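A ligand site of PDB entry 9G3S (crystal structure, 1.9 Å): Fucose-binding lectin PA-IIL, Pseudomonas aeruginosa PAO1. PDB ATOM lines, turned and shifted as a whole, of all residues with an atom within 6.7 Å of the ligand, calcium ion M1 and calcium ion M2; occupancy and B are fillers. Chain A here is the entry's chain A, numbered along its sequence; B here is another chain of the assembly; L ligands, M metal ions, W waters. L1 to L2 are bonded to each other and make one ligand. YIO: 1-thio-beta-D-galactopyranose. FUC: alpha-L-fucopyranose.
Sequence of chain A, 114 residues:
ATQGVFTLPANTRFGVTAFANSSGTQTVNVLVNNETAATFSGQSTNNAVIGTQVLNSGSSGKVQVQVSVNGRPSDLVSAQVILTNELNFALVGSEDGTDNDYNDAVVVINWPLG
The side-chain carboxylate of Asp 96 sits close to an oxygen (O2) of FUC L2, at 2.4 Å.
The backbone NH (N) of Ser 23 lies within hydrogen-bond range of an oxygen (O5) of FUC L2.
The side-chain hydroxyl (OG) of Ser 22 lies close to an oxygen (O5) of FUC L2, 3.4 Å away.
Of the 26 residues printed, 5 come within 4 Å of calcium ion M2.
Along chain A the residues within 4 Å of calcium ion M2 span positions 21 to 104.
CA of Gly 24 touches O6 of YIO L1, at 3.6 Å.
Ten residues have an atom within 4 Å of the ligand: Asn 21, Ser 22, Ser 23, Gly 24, Glu 95, Asp 96, Asp 99, Asp 101, Asp 104 and Gly 114 of chain B.
Four residues have an atom within 4 Å of calcium ion M1: Glu 95, Asp 99, Asp 101 and Asp 104.
Water W1 bridges an oxygen (O5) of YIO L1 and the backbone carbonyl oxygen (O) of Asp 96.
Water W2 lies within hydrogen-bond range of N of Thr 98 (3.0 Å), N of Asp 99 (3.1 Å) and S1 of YIO L1 (3.5 Å).
The side-chain carboxylate (OD2) of Asp 104 lies close to the backbone NH (N) of Asp 96 (2.8 Å).
N of Asn 21 lies close to O of Ser 44, 3.3 Å away.
N of Gly 97 sits close to OE2 of Glu 95, 2.8 Å away.
The side-chain carboxylate of Glu 95 sits close to the backbone NH of Asn 100, 3.3 Å away.
The side-chain carboxylate (OD2) of Asp 96 sits at hydrogen-bond distance from the side-chain amide nitrogen (NE2) of Gln 26 (2.9 Å).
The side-chain hydroxyl (OG) of Ser 22 sits at hydrogen-bond distance from the backbone NH (N) of Gly 24 (3.1 Å).
N of Ser 22 sits at hydrogen-bond distance from O of Ser 44.
The backbone carbonyl oxygen (O) of Gly 24 is in hydrogen-bond range of the side-chain amide nitrogen (NE2) of Gln 26 (3.2 Å).
Calcium ion M2 is bound by OD1 of Asp 104, 2.4 Å away.
O of Asn 21 is bound to calcium ion M2 (2.4 Å).
O of Gly 114 of chain B binds calcium ion M2, 2.4 Å away.
OD1 of Asn 103 binds calcium ion M2, at 2.4 Å.
Calcium ion M2 is bound by OD2 of Asp 101 (2.5 Å).
O4 of FUC L2 is bound to calcium ion M2.
O3 of FUC L2 is bound to calcium ion M2 (2.5 Å).
Calcium ion M2 has seven donor atoms within binding distance.
Slightly farther from calcium ion M2 lies OD1 of Asp 101 (2.9 Å).
Calcium ion M1 is bound by the side-chain carboxylate (OD1) of Asp 99 (2.3 Å), the side-chain carboxylate (OE2) of Glu 95 (2.4 Å), the side-chain carboxylate (OD1) of Asp 101 (2.4 Å), an oxygen (O3) of FUC L2 (2.4 Å), the side-chain carboxylate (OD2) of Asp 104 (2.4 Å), the side-chain carboxylate (OE1) of Glu 95 (2.5 Å), an oxygen (O2) of FUC L2 (2.5 Å) and the side-chain carboxylate (OD1) of Asp 104 (2.7 Å).
Calcium ion M1 has eight donor atoms within binding distance.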
ATOM      1  N   ASN A  21     -15.674  13.820  15.788  1.00  0.00           N
ATOM      2  CA  ASN A  21     -14.888  13.070  14.828  1.00  0.00           C
ATOM      3  C   ASN A  21     -15.420  11.635  14.686  1.00  0.00           C
ATOM      4  O   ASN A  21     -14.783  10.668  15.113  1.00  0.00           O
ATOM      5  CB  ASN A  21     -13.409  13.049  15.203  1.00  0.00           C
ATOM      6  CG  ASN A  21     -12.779  14.421  15.200  1.00  0.00           C
ATOM      7  OD1 ASN A  21     -12.268  14.874  14.168  1.00  0.00           O
ATOM      8  ND2 ASN A  21     -12.709  15.059  16.357  1.00  0.00           N
ATOM      9  N   SER A  22     -16.547  11.472  13.979  1.00  0.00           N
ATOM     10  CA  SER A  22     -17.235  10.191  13.879  1.00  0.00           C
ATOM     11  C   SER A  22     -18.368  10.294  12.854  1.00  0.00           C
ATOM     12  O   SER A  22     -18.926  11.382  12.630  1.00  0.00           O
ATOM     13  CB  SER A  22     -17.753   9.749  15.261  1.00  0.00           C
ATOM     14  OG  SER A  22     -18.538   8.563  15.198  1.00  0.00           O
ATOM     15  N   SER A  23     -18.690   9.161  12.212  1.00  0.00           N
ATOM     16  CA  SER A  23     -19.858   9.058  11.346  1.00  0.00           C
ATOM     17  C   SER A  23     -21.124   9.279  12.148  1.00  0.00           C
ATOM     18  O   SER A  23     -22.096   9.831  11.633  1.00  0.00           O
ATOM     19  CB  SER A  23     -19.922   7.725  10.639  1.00  0.00           C
ATOM     20  OG  SER A  23     -18.740   7.478   9.885  1.00  0.00           O
ATOM     21  N   GLY A  24     -21.102   8.863  13.421  1.00  0.00           N
ATOM     22  CA  GLY A  24     -22.282   8.920  14.273  1.00  0.00           C
ATOM     23  C   GLY A  24     -22.519  10.323  14.819  1.00  0.00           C
ATOM     24  O   GLY A  24     -21.568  11.036  15.162  1.00  0.00           O
ATOM     25  N   THR A  25     -23.802  10.708  14.931  1.00  0.00           N
ATOM     26  CA  THR A  25     -24.178  11.918  15.636  1.00  0.00           C
ATOM     27  C   THR A  25     -23.775  11.781  17.103  1.00  0.00           C
ATOM     28  O   THR A  25     -24.219  10.835  17.761  1.00  0.00           O
ATOM     29  CB  THR A  25     -25.680  12.192  15.515  1.00  0.00           C
ATOM     30  OG1 THR A  25     -25.892  12.429  14.136  1.00  0.00           O
ATOM     31  CG2 THR A  25     -26.110  13.441  16.274  1.00  0.00           C
ATOM     32  N   GLN A  26     -22.988  12.759  17.612  1.00  0.00           N
ATOM     33  CA  GLN A  26     -22.607  12.775  19.015  1.00  0.00           C
ATOM     34  C   GLN A  26     -23.541  13.661  19.816  1.00  0.00           C
ATOM     35  O   GLN A  26     -23.879  14.772  19.390  1.00  0.00           O
ATOM     36  CB  GLN A  26     -21.179  13.313  19.139  1.00  0.00           C
ATOM     37  CG  GLN A  26     -20.186  12.574  18.252  1.00  0.00           C
ATOM     38  CD  GLN A  26     -19.909  11.169  18.725  1.00  0.00           C
ATOM     39  OE1 GLN A  26     -19.660  10.938  19.909  1.00  0.00           O
ATOM     40  NE2 GLN A  26     -19.989  10.207  17.814  1.00  0.00           N
ATOM     41  N   SER A  44     -19.698  15.208  12.663  1.00  0.00           N
ATOM     42  CA  SER A  44     -18.614  15.659  11.815  1.00  0.00           C
ATOM     43  C   SER A  44     -17.554  14.587  11.864  1.00  0.00           C
ATOM     44  O   SER A  44     -17.350  14.040  12.936  1.00  0.00           O
ATOM     45  CB  SER A  44     -18.034  16.998  12.347  1.00  0.00           C
ATOM     46  OG  SER A  44     -16.839  17.400  11.648  1.00  0.00           O
ATOM     47  N   THR A  45     -16.793  14.405  10.773  1.00  0.00           N
ATOM     48  CA  THR A  45     -15.540  13.690  10.834  1.00  0.00           C
ATOM     49  C   THR A  45     -14.367  14.660  10.630  1.00  0.00           C
ATOM     50  O   THR A  45     -13.267  14.236  10.305  1.00  0.00           O
ATOM     51  CB  THR A  45     -15.500  12.564   9.791  1.00  0.00           C
ATOM     52  OG1 THR A  45     -15.795  13.137   8.527  1.00  0.00           O
ATOM     53  CG2 THR A  45     -16.486  11.447  10.082  1.00  0.00           C
ATOM     54  N   VAL A  69     -24.157   8.131  21.711  1.00  0.00           N
ATOM     55  CA  VAL A  69     -24.419   8.091  20.285  1.00  0.00           C
ATOM     56  C   VAL A  69     -25.670   7.246  20.102  1.00  0.00           C
ATOM     57  O   VAL A  69     -25.705   6.086  20.517  1.00  0.00           O
ATOM     58  CB  VAL A  69     -23.193   7.527  19.550  1.00  0.00           C
ATOM     59  CG1 VAL A  69     -23.413   7.448  18.041  1.00  0.00           C
ATOM     60  CG2 VAL A  69     -21.958   8.352  19.889  1.00  0.00           C
ATOM     61  N   ASN A  70     -26.728   7.876  19.589  1.00  0.00           N
ATOM     62  CA  ASN A  70     -27.985   7.191  19.358  1.00  0.00           C
ATOM     63  C   ASN A  70     -28.437   6.512  20.647  1.00  0.00           C
ATOM     64  O   ASN A  70     -29.025   5.429  20.610  1.00  0.00           O
ATOM     65  CB  ASN A  70     -27.786   6.210  18.200  1.00  0.00           C
ATOM     66  CG  ASN A  70     -28.975   6.172  17.273  1.00  0.00           C
ATOM     67  OD1 ASN A  70     -29.999   6.810  17.538  1.00  0.00           O
ATOM     68  ND2 ASN A  70     -28.841   5.428  16.185  1.00  0.00           N
ATOM     69  N   ARG A  72     -26.512   5.308  23.176  1.00  0.00           N
ATOM     70  CA  ARG A  72     -25.538   4.419  23.807  1.00  0.00           C
ATOM     71  C   ARG A  72     -24.400   5.213  24.446  1.00  0.00           C
ATOM     72  O   ARG A  72     -23.696   5.942  23.741  1.00  0.00           O
ATOM     73  CB  ARG A  72     -24.936   3.546  22.711  1.00  0.00           C
ATOM     74  CG  ARG A  72     -25.916   2.673  21.949  1.00  0.00           C
ATOM     75  CD  ARG A  72     -25.137   1.738  21.046  1.00  0.00           C
ATOM     76  NE  ARG A  72     -24.364   2.413  20.002  1.00  0.00           N
ATOM     77  CZ  ARG A  72     -24.813   2.959  18.880  1.00  0.00           C
ATOM     78  NH1 ARG A  72     -26.069   2.761  18.453  1.00  0.00           N
ATOM     79  NH2 ARG A  72     -23.996   3.686  18.150  1.00  0.00           N
ATOM     80  N   SER A  94     -13.827  10.328  24.048  1.00  0.00           N
ATOM     81  CA  SER A  94     -14.899   9.353  24.044  1.00  0.00           C
ATOM     82  C   SER A  94     -14.790   8.459  22.810  1.00  0.00           C
ATOM     83  O   SER A  94     -14.389   8.902  21.725  1.00  0.00           O
ATOM     84  CB  SER A  94     -16.203  10.073  24.177  1.00  0.00           C
ATOM     85  OG  SER A  94     -16.580  10.757  22.995  1.00  0.00           O
ATOM     86  N   GLU A  95     -15.154   7.180  22.990  1.00  0.00           N
ATOM     87  CA  GLU A  95     -15.133   6.170  21.949  1.00  0.00           C
ATOM     88  C   GLU A  95     -16.528   5.566  21.808  1.00  0.00           C
ATOM     89  O   GLU A  95     -17.071   5.084  22.799  1.00  0.00           O
ATOM     90  CB  GLU A  95     -14.125   5.071  22.300  1.00  0.00           C
ATOM     91  CG  GLU A  95     -13.993   3.975  21.255  1.00  0.00           C
ATOM     92  CD  GLU A  95     -13.749   4.478  19.848  1.00  0.00           C
ATOM     93  OE1 GLU A  95     -12.806   5.282  19.659  1.00  0.00           O
ATOM     94  OE2 GLU A  95     -14.544   4.157  18.935  1.00  0.00           O
ATOM     95  N   ASP A  96     -17.072   5.616  20.585  1.00  0.00           N
ATOM     96  CA  ASP A  96     -18.372   5.062  20.257  1.00  0.00           C
ATOM     97  C   ASP A  96     -18.312   3.694  19.556  1.00  0.00           C
ATOM     98  O   ASP A  96     -19.349   3.096  19.288  1.00  0.00           O
ATOM     99  CB  ASP A  96     -19.178   6.019  19.408  1.00  0.00           C
ATOM    100  CG  ASP A  96     -18.652   6.351  18.006  1.00  0.00           C
ATOM    101  OD1 ASP A  96     -17.900   5.544  17.399  1.00  0.00           O
ATOM    102  OD2 ASP A  96     -19.005   7.454  17.514  1.00  0.00           O
ATOM    103  N   GLY A  97     -17.111   3.183  19.255  1.00  0.00           N
ATOM    104  CA  GLY A  97     -16.971   2.023  18.372  1.00  0.00           C
ATOM    105  C   GLY A  97     -15.825   1.122  18.826  1.00  0.00           C
ATOM    106  O   GLY A  97     -15.636   0.915  20.014  1.00  0.00           O
ATOM    107  N   THR A  98     -14.994   0.668  17.864  1.00  0.00           N
ATOM    108  CA  THR A  98     -14.018  -0.376  18.096  1.00  0.00           C
ATOM    109  C   THR A  98     -12.607   0.097  17.782  1.00  0.00           C
ATOM    110  O   THR A  98     -11.668  -0.572  18.177  1.00  0.00           O
ATOM    111  CB  THR A  98     -14.344  -1.613  17.254  1.00  0.00           C
ATOM    112  OG1 THR A  98     -14.419  -1.179  15.896  1.00  0.00           O
ATOM    113  CG2 THR A  98     -15.682  -2.232  17.598  1.00  0.00           C
ATOM    114  N   ASP A  99     -12.441   1.230  17.110  1.00  0.00           N
ATOM    115  CA  ASP A  99     -11.118   1.624  16.649  1.00  0.00           C
ATOM    116  C   ASP A  99     -10.262   2.269  17.739  1.00  0.00           C
ATOM    117  O   ASP A  99      -9.085   2.450  17.539  1.00  0.00           O
ATOM    118  CB  ASP A  99     -11.176   2.507  15.416  1.00  0.00           C
ATOM    119  CG  ASP A  99     -11.764   3.907  15.566  1.00  0.00           C
ATOM    120  OD1 ASP A  99     -12.345   4.213  16.629  1.00  0.00           O
ATOM    121  OD2 ASP A  99     -11.651   4.675  14.605  1.00  0.00           O
ATOM    122  N   ASN A 100     -10.876   2.694  18.849  1.00  0.00           N
ATOM    123  CA  ASN A 100     -10.173   3.266  19.981  1.00  0.00           C
ATOM    124  C   ASN A 100      -9.308   4.475  19.597  1.00  0.00           C
ATOM    125  O   ASN A 100      -8.233   4.629  20.150  1.00  0.00           O
ATOM    126  CB  ASN A 100      -9.355   2.212  20.696  1.00  0.00           C
ATOM    127  CG  ASN A 100     -10.244   1.135  21.258  1.00  0.00           C
ATOM    128  OD1 ASN A 100     -11.468   1.313  21.360  1.00  0.00           O
ATOM    129  ND2 ASN A 100      -9.673  -0.004  21.587  1.00  0.00           N
ATOM    130  N   ASP A 101      -9.853   5.396  18.787  1.00  0.00           N
ATOM    131  CA  ASP A 101      -9.219   6.693  18.566  1.00  0.00           C
ATOM    132  C   ASP A 101      -9.628   7.682  19.684  1.00  0.00           C
ATOM    133  O   ASP A 101      -8.913   8.654  19.946  1.00  0.00           O
ATOM    134  CB  ASP A 101      -9.405   7.205  17.152  1.00  0.00           C
ATOM    135  CG  ASP A 101     -10.816   7.495  16.658  1.00  0.00           C
ATOM    136  OD1 ASP A 101     -11.804   7.260  17.390  1.00  0.00           O
ATOM    137  OD2 ASP A 101     -10.921   8.007  15.533  1.00  0.00           O
ATOM    138  N   TYR A 102     -10.732   7.390  20.398  1.00  0.00           N
ATOM    139  CA  TYR A 102     -11.153   8.165  21.565  1.00  0.00           C
ATOM    140  C   TYR A 102     -11.408   9.643  21.213  1.00  0.00           C
ATOM    141  O   TYR A 102     -11.401  10.508  22.080  1.00  0.00           O
ATOM    142  CB  TYR A 102     -10.193   7.961  22.752  1.00  0.00           C
ATOM    143  CG  TYR A 102     -10.622   6.702  23.493  1.00  0.00           C
ATOM    144  CD1 TYR A 102     -10.197   5.455  23.057  1.00  0.00           C
ATOM    145  CD2 TYR A 102     -11.589   6.743  24.488  1.00  0.00           C
ATOM    146  CE1 TYR A 102     -10.660   4.295  23.650  1.00  0.00           C
ATOM    147  CE2 TYR A 102     -12.026   5.592  25.119  1.00  0.00           C
ATOM    148  CZ  TYR A 102     -11.589   4.352  24.666  1.00  0.00           C
ATOM    149  OH  TYR A 102     -12.066   3.202  25.258  1.00  0.00           O
ATOM    150  N   ASN A 103     -11.683   9.951  19.939  1.00  0.00           N
ATOM    151  CA  ASN A 103     -11.852  11.333  19.519  1.00  0.00           C
ATOM    152  C   ASN A 103     -13.290  11.574  19.035  1.00  0.00           C
ATOM    153  O   ASN A 103     -13.584  12.590  18.422  1.00  0.00           O
ATOM    154  CB  ASN A 103     -10.827  11.691  18.456  1.00  0.00           C
ATOM    155  CG  ASN A 103     -11.161  11.064  17.134  1.00  0.00           C
ATOM    156  OD1 ASN A 103     -12.165  10.359  17.035  1.00  0.00           O
ATOM    157  ND2 ASN A 103     -10.364  11.342  16.116  1.00  0.00           N
ATOM    158  N   ASP A 104     -14.184  10.616  19.298  1.00  0.00           N
ATOM    159  CA  ASP A 104     -15.468  10.623  18.591  1.00  0.00           C
ATOM    160  C   ASP A 104     -16.274  11.853  18.961  1.00  0.00           C
ATOM    161  O   ASP A 104     -16.819  12.505  18.068  1.00  0.00           O
ATOM    162  CB  ASP A 104     -16.192   9.302  18.744  1.00  0.00           C
ATOM    163  CG  ASP A 104     -15.396   8.129  18.174  1.00  0.00           C
ATOM    164  OD1 ASP A 104     -14.727   8.323  17.122  1.00  0.00           O
ATOM    165  OD2 ASP A 104     -15.404   7.057  18.808  1.00  0.00           O
ATOM    166  N   ALA A 105     -16.361  12.101  20.276  1.00  0.00           N
ATOM    167  CA  ALA A 105     -16.602  13.447  20.804  1.00  0.00           C
ATOM    168  C   ALA A 105     -15.413  13.795  21.710  1.00  0.00           C
ATOM    169  O   ALA A 105     -15.023  13.000  22.574  1.00  0.00           O
ATOM    170  CB  ALA A 105     -17.907  13.538  21.569  1.00  0.00           C
ATOM    171  N   PRO B 112      -5.753  12.523  17.243  1.00  0.00           N
ATOM    172  CA  PRO B 112      -6.093  12.563  15.815  1.00  0.00           C
ATOM    173  C   PRO B 112      -7.511  13.061  15.529  1.00  0.00           C
ATOM    174  O   PRO B 112      -8.381  13.100  16.413  1.00  0.00           O
ATOM    175  CB  PRO B 112      -5.926  11.065  15.438  1.00  0.00           C
ATOM    176  CG  PRO B 112      -6.443  10.361  16.693  1.00  0.00           C
ATOM    177  CD  PRO B 112      -5.796  11.154  17.802  1.00  0.00           C
ATOM    178  N   LEU B 113      -7.755  13.374  14.252  1.00  0.00           N
ATOM    179  CA  LEU B 113      -9.113  13.671  13.804  1.00  0.00           C
ATOM    180  C   LEU B 113      -9.697  12.487  13.045  1.00  0.00           C
ATOM    181  O   LEU B 113      -8.937  11.584  12.684  1.00  0.00           O
ATOM    182  CB  LEU B 113      -8.995  14.886  12.915  1.00  0.00           C
ATOM    183  CG  LEU B 113      -8.344  16.125  13.552  1.00  0.00           C
ATOM    184  CD1 LEU B 113      -8.530  17.249  12.554  1.00  0.00           C
ATOM    185  CD2 LEU B 113      -8.928  16.474  14.915  1.00  0.00           C
ATOM    186  N   GLY B 114     -11.019  12.520  12.756  1.00  0.00           N
ATOM    187  CA  GLY B 114     -11.657  11.594  11.821  1.00  0.00           C
ATOM    188  C   GLY B 114     -12.380  10.456  12.522  1.00  0.00           C
ATOM    189  O   GLY B 114     -12.062  10.193  13.718  1.00  0.00           O
ATOM    190  OXT GLY B 114     -13.243   9.797  11.846  1.00  0.00           O
HETATM  191  C1  YIO L   1     -18.812   4.186  12.895  1.00  0.00           C
HETATM  192  C2  YIO L   1     -19.207   2.838  12.345  1.00  0.00           C
HETATM  193  C3  YIO L   1     -20.644   2.948  11.861  1.00  0.00           C
HETATM  194  C4  YIO L   1     -21.489   3.312  13.048  1.00  0.00           C
HETATM  195  C5  YIO L   1     -21.004   4.658  13.597  1.00  0.00           C
HETATM  196  C6  YIO L   1     -21.755   5.129  14.831  1.00  0.00           C
HETATM  197  O2  YIO L   1     -18.392   2.410  11.258  1.00  0.00           O
HETATM  198  O3  YIO L   1     -21.029   1.722  11.278  1.00  0.00           O
HETATM  199  O4  YIO L   1     -21.305   2.328  14.073  1.00  0.00           O
HETATM  200  O5  YIO L   1     -19.631   4.487  13.999  1.00  0.00           O
HETATM  201  O6  YIO L   1     -23.097   5.417  14.466  1.00  0.00           O
HETATM  202  S1  YIO L   1     -17.097   4.167  13.478  1.00  0.00           S
HETATM  203  C1  FUC L   2     -16.913   5.913  13.959  1.00  0.00           C
HETATM  204  C2  FUC L   2     -15.786   6.202  14.947  1.00  0.00           C
HETATM  205  C3  FUC L   2     -14.453   6.014  14.240  1.00  0.00           C
HETATM  206  C4  FUC L   2     -14.392   6.830  12.957  1.00  0.00           C
HETATM  207  C5  FUC L   2     -15.612   6.531  12.085  1.00  0.00           C
HETATM  208  C6  FUC L   2     -15.668   7.386  10.841  1.00  0.00           C
HETATM  209  O2  FUC L   2     -15.846   5.366  16.116  1.00  0.00           O
HETATM  210  O3  FUC L   2     -13.406   6.418  15.109  1.00  0.00           O
HETATM  211  O4  FUC L   2     -14.376   8.224  13.308  1.00  0.00           O
HETATM  212  O5  FUC L   2     -16.816   6.776  12.839  1.00  0.00           O
HETATM  213 CA    CA M   1     -13.771   5.869  17.450  1.00  0.00          CA
HETATM  214 CA    CA M   2     -13.227   8.916  15.407  1.00  0.00          CA
HETATM  215  O   HOH W   1     -19.472   3.067  16.255  1.00  0.00           O
HETATM  216  O   HOH W   2     -14.838   2.566  15.586  1.00  0.00           O
